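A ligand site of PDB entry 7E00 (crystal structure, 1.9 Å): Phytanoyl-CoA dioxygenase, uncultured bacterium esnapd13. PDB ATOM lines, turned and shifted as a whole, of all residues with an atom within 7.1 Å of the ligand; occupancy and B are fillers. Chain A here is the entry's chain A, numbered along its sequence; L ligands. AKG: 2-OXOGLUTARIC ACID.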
ATOM      1  N   GLU A  35       9.981  20.837  22.177  1.00  0.00           N
ATOM      2  CA  GLU A  35       8.938  20.346  21.361  1.00  0.00           C
ATOM      3  C   GLU A  35       9.245  20.550  19.856  1.00  0.00           C
ATOM      4  O   GLU A  35       8.859  19.718  19.072  1.00  0.00           O
ATOM      5  CB  GLU A  35       7.591  21.011  21.759  1.00  0.00           C
ATOM      6  CG  GLU A  35       6.476  20.622  20.823  1.00  0.00           C
ATOM      7  CD  GLU A  35       6.245  19.085  20.848  1.00  0.00           C
ATOM      8  OE1 GLU A  35       6.184  18.528  22.001  1.00  0.00           O
ATOM      9  OE2 GLU A  35       6.186  18.473  19.742  1.00  0.00           O
ATOM     10  N   LEU A  37      12.229  20.374  18.593  1.00  0.00           N
ATOM     11  CA  LEU A  37      13.167  19.346  18.348  1.00  0.00           C
ATOM     12  C   LEU A  37      12.529  17.947  18.310  1.00  0.00           C
ATOM     13  O   LEU A  37      12.868  17.103  17.439  1.00  0.00           O
ATOM     14  CB  LEU A  37      14.253  19.369  19.340  1.00  0.00           C
ATOM     15  CG  LEU A  37      15.156  20.633  19.431  1.00  0.00           C
ATOM     16  CD1 LEU A  37      16.296  20.297  20.355  1.00  0.00           C
ATOM     17  CD2 LEU A  37      15.698  21.065  18.085  1.00  0.00           C
ATOM     18  N   ARG A  38      11.575  17.709  19.204  1.00  0.00           N
ATOM     19  CA  ARG A  38      10.807  16.443  19.134  1.00  0.00           C
ATOM     20  C   ARG A  38      10.027  16.267  17.794  1.00  0.00           C
ATOM     21  O   ARG A  38      10.006  15.191  17.230  1.00  0.00           O
ATOM     22  CB  ARG A  38       9.850  16.360  20.299  1.00  0.00           C
ATOM     23  CG  ARG A  38      10.523  16.169  21.645  1.00  0.00           C
ATOM     24  CD  ARG A  38       9.580  16.413  22.872  1.00  0.00           C
ATOM     25  NE  ARG A  38       8.554  15.414  22.888  1.00  0.00           N
ATOM     26  CZ  ARG A  38       8.671  14.180  23.393  1.00  0.00           C
ATOM     27  NH1 ARG A  38       9.776  13.724  23.977  1.00  0.00           N
ATOM     28  NH2 ARG A  38       7.643  13.350  23.273  1.00  0.00           N
ATOM     29  N   ALA A  39       9.367  17.329  17.294  1.00  0.00           N
ATOM     30  CA  ALA A  39       8.663  17.247  16.026  1.00  0.00           C
ATOM     31  C   ALA A  39       9.637  16.921  14.904  1.00  0.00           C
ATOM     32  O   ALA A  39       9.338  16.127  14.012  1.00  0.00           O
ATOM     33  CB  ALA A  39       7.872  18.563  15.727  1.00  0.00           C
ATOM     34  N   GLU A  40      10.823  17.526  14.928  1.00  0.00           N
ATOM     35  CA  GLU A  40      11.756  17.275  13.846  1.00  0.00           C
ATOM     36  C   GLU A  40      12.337  15.891  13.979  1.00  0.00           C
ATOM     37  O   GLU A  40      12.587  15.201  12.997  1.00  0.00           O
ATOM     38  CB  GLU A  40      12.853  18.327  13.886  1.00  0.00           C
ATOM     39  CG  GLU A  40      13.719  18.396  12.654  1.00  0.00           C
ATOM     40  CD  GLU A  40      13.011  18.942  11.434  1.00  0.00           C
ATOM     41  OE1 GLU A  40      11.865  19.329  11.502  1.00  0.00           O
ATOM     42  OE2 GLU A  40      13.603  18.925  10.363  1.00  0.00           O
ATOM     43  N   ALA A  41      12.531  15.441  15.176  1.00  0.00           N
ATOM     44  CA  ALA A  41      13.022  14.086  15.372  1.00  0.00           C
ATOM     45  C   ALA A  41      12.027  13.100  14.763  1.00  0.00           C
ATOM     46  O   ALA A  41      12.392  12.109  14.053  1.00  0.00           O
ATOM     47  CB  ALA A  41      13.143  13.825  16.848  1.00  0.00           C
ATOM     48  N   ALA A  42      10.755  13.369  15.042  1.00  0.00           N
ATOM     49  CA  ALA A  42       9.704  12.482  14.505  1.00  0.00           C
ATOM     50  C   ALA A  42       9.734  12.482  12.978  1.00  0.00           C
ATOM     51  O   ALA A  42       9.597  11.418  12.380  1.00  0.00           O
ATOM     52  CB  ALA A  42       8.308  12.873  15.076  1.00  0.00           C
ATOM     53  N   GLN A  43       9.958  13.622  12.339  1.00  0.00           N
ATOM     54  CA  GLN A  43      10.082  13.696  10.873  1.00  0.00           C
ATOM     55  C   GLN A  43      11.252  12.865  10.353  1.00  0.00           C
ATOM     56  O   GLN A  43      11.149  12.142   9.325  1.00  0.00           O
ATOM     57  CB  GLN A  43      10.405  15.119  10.408  1.00  0.00           C
ATOM     58  CG  GLN A  43       9.316  16.043   9.994  1.00  0.00           C
ATOM     59  CD  GLN A  43       8.382  15.381   9.004  1.00  0.00           C
ATOM     60  OE1 GLN A  43       7.183  15.573   9.116  1.00  0.00           O
ATOM     61  NE2 GLN A  43       8.925  14.555   8.070  1.00  0.00           N
ATOM     62  N   PHE A  45      12.684  10.281  11.853  1.00  0.00           N
ATOM     63  CA  PHE A  45      12.407   8.877  12.005  1.00  0.00           C
ATOM     64  C   PHE A  45      11.445   8.446  10.887  1.00  0.00           C
ATOM     65  O   PHE A  45      11.599   7.387  10.346  1.00  0.00           O
ATOM     66  CB  PHE A  45      11.841   8.558  13.365  1.00  0.00           C
ATOM     67  CG  PHE A  45      12.863   8.470  14.437  1.00  0.00           C
ATOM     68  CD1 PHE A  45      13.769   7.417  14.464  1.00  0.00           C
ATOM     69  CD2 PHE A  45      12.884   9.348  15.475  1.00  0.00           C
ATOM     70  CE1 PHE A  45      14.701   7.289  15.492  1.00  0.00           C
ATOM     71  CE2 PHE A  45      13.806   9.229  16.494  1.00  0.00           C
ATOM     72  CZ  PHE A  45      14.723   8.196  16.527  1.00  0.00           C
ATOM     73  N   VAL A  61      11.763   2.085  15.618  1.00  0.00           N
ATOM     74  CA  VAL A  61      12.853   3.044  15.636  1.00  0.00           C
ATOM     75  C   VAL A  61      13.784   2.884  16.871  1.00  0.00           C
ATOM     76  O   VAL A  61      13.347   2.943  18.017  1.00  0.00           O
ATOM     77  CB  VAL A  61      12.244   4.444  15.445  1.00  0.00           C
ATOM     78  CG1 VAL A  61      11.343   4.411  14.202  1.00  0.00           C
ATOM     79  CG2 VAL A  61      11.430   4.923  16.652  1.00  0.00           C
ATOM     80  N   ILE A 102      19.964  10.484  16.905  1.00  0.00           N
ATOM     81  CA  ILE A 102      18.812  10.618  17.838  1.00  0.00           C
ATOM     82  C   ILE A 102      18.480   9.151  18.257  1.00  0.00           C
ATOM     83  O   ILE A 102      18.241   8.285  17.383  1.00  0.00           O
ATOM     84  CB  ILE A 102      17.624  11.252  17.189  1.00  0.00           C
ATOM     85  CG1 ILE A 102      18.008  12.629  16.669  1.00  0.00           C
ATOM     86  CG2 ILE A 102      16.438  11.392  18.167  1.00  0.00           C
ATOM     87  CD1 ILE A 102      16.910  13.308  15.993  1.00  0.00           C
ATOM     88  N   ASN A 103      18.653   8.889  19.532  1.00  0.00           N
ATOM     89  CA  ASN A 103      18.449   7.502  20.108  1.00  0.00           C
ATOM     90  C   ASN A 103      17.160   7.586  20.883  1.00  0.00           C
ATOM     91  O   ASN A 103      17.045   8.323  21.871  1.00  0.00           O
ATOM     92  CB  ASN A 103      19.629   7.040  20.996  1.00  0.00           C
ATOM     93  CG  ASN A 103      20.851   6.532  20.177  1.00  0.00           C
ATOM     94  OD1 ASN A 103      20.794   6.283  18.959  1.00  0.00           O
ATOM     95  ND2 ASN A 103      21.944   6.318  20.874  1.00  0.00           N
ATOM     96  N   ALA A 104      16.145   6.935  20.309  1.00  0.00           N
ATOM     97  CA  ALA A 104      14.812   6.951  20.873  1.00  0.00           C
ATOM     98  C   ALA A 104      14.870   5.793  21.857  1.00  0.00           C
ATOM     99  O   ALA A 104      15.064   4.676  21.467  1.00  0.00           O
ATOM    100  CB  ALA A 104      13.797   6.683  19.759  1.00  0.00           C
ATOM    101  N   LYS A 105      14.825   6.002  23.144  1.00  0.00           N
ATOM    102  CA  LYS A 105      14.861   4.792  23.994  1.00  0.00           C
ATOM    103  C   LYS A 105      13.395   4.631  24.329  1.00  0.00           C
ATOM    104  O   LYS A 105      12.930   5.243  25.249  1.00  0.00           O
ATOM    105  CB  LYS A 105      15.818   4.918  25.179  1.00  0.00           C
ATOM    106  CG  LYS A 105      15.930   3.644  26.013  1.00  0.00           C
ATOM    107  CD  LYS A 105      17.351   3.202  26.325  1.00  0.00           C
ATOM    108  CE  LYS A 105      17.833   2.078  25.416  1.00  0.00           C
ATOM    109  NZ  LYS A 105      18.927   1.263  26.033  1.00  0.00           N
ATOM    110  N   ARG A 106      12.666   3.961  23.430  1.00  0.00           N
ATOM    111  CA  ARG A 106      11.190   3.884  23.465  1.00  0.00           C
ATOM    112  C   ARG A 106      10.737   3.257  24.794  1.00  0.00           C
ATOM    113  O   ARG A 106      11.400   2.369  25.329  1.00  0.00           O
ATOM    114  CB  ARG A 106      10.646   3.003  22.303  1.00  0.00           C
ATOM    115  CG  ARG A 106      10.527   3.571  20.891  1.00  0.00           C
ATOM    116  CD  ARG A 106      11.185   4.905  20.668  1.00  0.00           C
ATOM    117  NE  ARG A 106      10.264   5.982  21.008  1.00  0.00           N
ATOM    118  CZ  ARG A 106       9.438   6.575  20.147  1.00  0.00           C
ATOM    119  NH1 ARG A 106       9.405   6.247  18.850  1.00  0.00           N
ATOM    120  NH2 ARG A 106       8.640   7.528  20.610  1.00  0.00           N
ATOM    121  N   ALA A 107       9.606   3.741  25.277  1.00  0.00           N
ATOM    122  CA  ALA A 107       8.976   3.292  26.516  1.00  0.00           C
ATOM    123  C   ALA A 107       8.802   1.787  26.915  1.00  0.00           C
ATOM    124  O   ALA A 107       8.475   1.573  28.078  1.00  0.00           O
ATOM    125  CB  ALA A 107       7.630   4.001  26.626  1.00  0.00           C
ATOM    126  N   LEU A 140      15.292  15.135  25.414  1.00  0.00           N
ATOM    127  CA  LEU A 140      13.984  15.461  24.872  1.00  0.00           C
ATOM    128  C   LEU A 140      12.851  15.045  25.838  1.00  0.00           C
ATOM    129  O   LEU A 140      11.692  15.460  25.662  1.00  0.00           O
ATOM    130  CB  LEU A 140      13.791  14.756  23.561  1.00  0.00           C
ATOM    131  CG  LEU A 140      14.719  15.071  22.400  1.00  0.00           C
ATOM    132  CD1 LEU A 140      14.350  14.238  21.178  1.00  0.00           C
ATOM    133  CD2 LEU A 140      14.620  16.542  22.076  1.00  0.00           C
ATOM    134  N   ASP A 141      13.203  14.196  26.792  1.00  0.00           N
ATOM    135  CA  ASP A 141      12.298  13.753  27.879  1.00  0.00           C
ATOM    136  C   ASP A 141      13.102  13.934  29.174  1.00  0.00           C
ATOM    137  O   ASP A 141      14.352  13.822  29.179  1.00  0.00           O
ATOM    138  CB  ASP A 141      11.966  12.298  27.668  1.00  0.00           C
ATOM    139  CG  ASP A 141      11.199  12.035  26.375  1.00  0.00           C
ATOM    140  OD1 ASP A 141      10.020  12.405  26.357  1.00  0.00           O
ATOM    141  OD2 ASP A 141      11.713  11.503  25.349  1.00  0.00           O
ATOM    142  N   ARG A 204      13.791  17.608  31.048  1.00  0.00           N
ATOM    143  CA  ARG A 204      13.673  17.916  29.649  1.00  0.00           C
ATOM    144  C   ARG A 204      14.410  19.250  29.343  1.00  0.00           C
ATOM    145  O   ARG A 204      14.306  20.262  30.043  1.00  0.00           O
ATOM    146  CB  ARG A 204      12.193  17.978  29.328  1.00  0.00           C
ATOM    147  CG  ARG A 204      11.866  18.572  28.006  1.00  0.00           C
ATOM    148  CD  ARG A 204      10.351  18.507  27.833  1.00  0.00           C
ATOM    149  NE  ARG A 204       9.950  17.170  27.460  1.00  0.00           N
ATOM    150  CZ  ARG A 204       8.713  16.807  27.209  1.00  0.00           C
ATOM    151  NH1 ARG A 204       7.731  17.677  27.342  1.00  0.00           N
ATOM    152  NH2 ARG A 204       8.460  15.557  26.847  1.00  0.00           N
ATOM    153  N   PHE A 225       7.736   5.541  30.121  1.00  0.00           N
ATOM    154  CA  PHE A 225       8.168   6.821  29.550  1.00  0.00           C
ATOM    155  C   PHE A 225       9.297   6.660  28.532  1.00  0.00           C
ATOM    156  O   PHE A 225      10.196   5.852  28.711  1.00  0.00           O
ATOM    157  CB  PHE A 225       8.678   7.681  30.689  1.00  0.00           C
ATOM    158  CG  PHE A 225       7.683   7.855  31.787  1.00  0.00           C
ATOM    159  CD1 PHE A 225       6.390   8.335  31.503  1.00  0.00           C
ATOM    160  CD2 PHE A 225       7.999   7.492  33.100  1.00  0.00           C
ATOM    161  CE1 PHE A 225       5.451   8.479  32.514  1.00  0.00           C
ATOM    162  CE2 PHE A 225       7.061   7.646  34.110  1.00  0.00           C
ATOM    163  CZ  PHE A 225       5.797   8.144  33.820  1.00  0.00           C
ATOM    164  N   ASP A 226       9.259   7.447  27.456  1.00  0.00           N
ATOM    165  CA  ASP A 226      10.372   7.462  26.486  1.00  0.00           C
ATOM    166  C   ASP A 226      11.613   8.176  27.061  1.00  0.00           C
ATOM    167  O   ASP A 226      11.544   8.914  28.083  1.00  0.00           O
ATOM    168  CB  ASP A 226       9.975   8.152  25.198  1.00  0.00           C
ATOM    169  CG  ASP A 226       8.773   7.518  24.519  1.00  0.00           C
ATOM    170  OD1 ASP A 226       8.773   6.285  24.219  1.00  0.00           O
ATOM    171  OD2 ASP A 226       7.853   8.299  24.264  1.00  0.00           O
ATOM    172  N   ARG A 227      12.756   7.940  26.443  1.00  0.00           N
ATOM    173  CA  ARG A 227      13.953   8.641  26.863  1.00  0.00           C
ATOM    174  C   ARG A 227      14.678   9.028  25.534  1.00  0.00           C
ATOM    175  O   ARG A 227      15.770   8.519  25.212  1.00  0.00           O
ATOM    176  CB  ARG A 227      14.848   7.746  27.740  1.00  0.00           C
ATOM    177  CG  ARG A 227      16.083   8.466  28.275  1.00  0.00           C
ATOM    178  CD  ARG A 227      17.337   7.627  28.129  1.00  0.00           C
ATOM    179  NE  ARG A 227      17.740   7.435  26.725  1.00  0.00           N
ATOM    180  CZ  ARG A 227      18.841   6.796  26.290  1.00  0.00           C
ATOM    181  NH1 ARG A 227      19.735   6.258  27.116  1.00  0.00           N
ATOM    182  NH2 ARG A 227      19.080   6.679  24.986  1.00  0.00           N
ATOM    183  N   GLY A 228      14.040   9.939  24.821  1.00  0.00           N
ATOM    184  CA  GLY A 228      14.612  10.479  23.572  1.00  0.00           C
ATOM    185  C   GLY A 228      15.827  11.348  23.854  1.00  0.00           C
ATOM    186  O   GLY A 228      15.761  12.271  24.697  1.00  0.00           O
ATOM    187  N   LEU A 229      16.941  11.039  23.196  1.00  0.00           N
ATOM    188  CA  LEU A 229      18.149  11.920  23.284  1.00  0.00           C
ATOM    189  C   LEU A 229      18.604  12.332  21.902  1.00  0.00           C
ATOM    190  O   LEU A 229      18.648  11.486  21.015  1.00  0.00           O
ATOM    191  CB  LEU A 229      19.326  11.163  23.904  1.00  0.00           C
ATOM    192  CG  LEU A 229      19.105  10.628  25.333  1.00  0.00           C
ATOM    193  CD1 LEU A 229      20.353   9.854  25.679  1.00  0.00           C
ATOM    194  CD2 LEU A 229      18.904  11.738  26.302  1.00  0.00           C
HETATM  195  C1  AKG L   1      10.187  11.561  18.469  1.00  0.00           C
HETATM  196  O1  AKG L   1      10.006  10.692  17.576  1.00  0.00           O
HETATM  197  O2  AKG L   1       9.499  12.625  18.541  1.00  0.00           O
HETATM  198  C2  AKG L   1      11.234  11.336  19.478  1.00  0.00           C
HETATM  199  O5  AKG L   1      12.264  10.639  19.273  1.00  0.00           O
HETATM  200  C3  AKG L   1      10.954  12.058  20.798  1.00  0.00           C
HETATM  201  C4  AKG L   1      11.860  11.461  21.860  1.00  0.00           C
HETATM  202  C5  AKG L   1      11.386  10.092  22.313  1.00  0.00           C
HETATM  203  O3  AKG L   1      11.888   8.929  21.972  1.00  0.00           O
HETATM  204  O4  AKG L   1      10.436  10.305  23.086  1.00  0.00           O
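The guanidinium group of Arg 106 lies within salt-bridge range of an oxygen (O3) of the ligand, 3.5 Å away. O of Arg 38 lies close to O2 of the ligand (2.9 Å). The guanidinium group (NH1) of Arg 38 lies within salt-bridge range of an oxygen (O4) of the ligand. OD2 of Asp 141 sits close to O4 of the ligand.
The side-chain carboxylate of Asp 226 sits close to an oxygen (O4) of the ligand (3.5 Å). Residues that only touch the ligand: Gly 228 (3.4 Å), Phe 45 (3.5 Å), Ala 42 (3.6 Å), Ala 104 (3.7 Å) and Leu 140 (3.8 Å). Hydrophobic or aromatic side chains that line the ligand: Ala 42, Phe 45, Ala 104 and Leu 140. Of the 24 residues printed, 9 come within 4 Å of the ligand. Along chain A the residues within 4 Å of the ligand span positions 38 to 228.
The backbone carbonyl oxygen (O) of Gly 228 is in hydrogen-bond range of the backbone NH (N) of Leu 140, at 3.0 Å. NH1 of Arg 38 sits at hydrogen-bond distance from O of Leu 140 (3.1 Å). The backbone carbonyl oxygen of Leu 140 lies within hydrogen-bond range of the guanidinium group of Arg 204 (3.0 Å). The side-chain carboxylate (OD1) of Asp 141 lies within salt-bridge range of the guanidinium group (NH2) of Arg 204. The side-chain carboxylate of Asp 141 is in salt-bridge range of the guanidinium group of Arg 38 (2.7 Å). The side-chain carboxylate (OD2) of Asp 141 sits at hydrogen-bond distance from the backbone NH (N) of Gly 228 (2.9 Å). The side-chain carboxylate (OD1) of Asp 226 lies within salt-bridge range of the guanidinium group (NE) of Arg 106 (3.6 Å). The backbone NH (N) of Ala 107 lies within hydrogen-bond range of the side-chain carboxylate (OD1) of Asp 226, at 2.9 Å.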
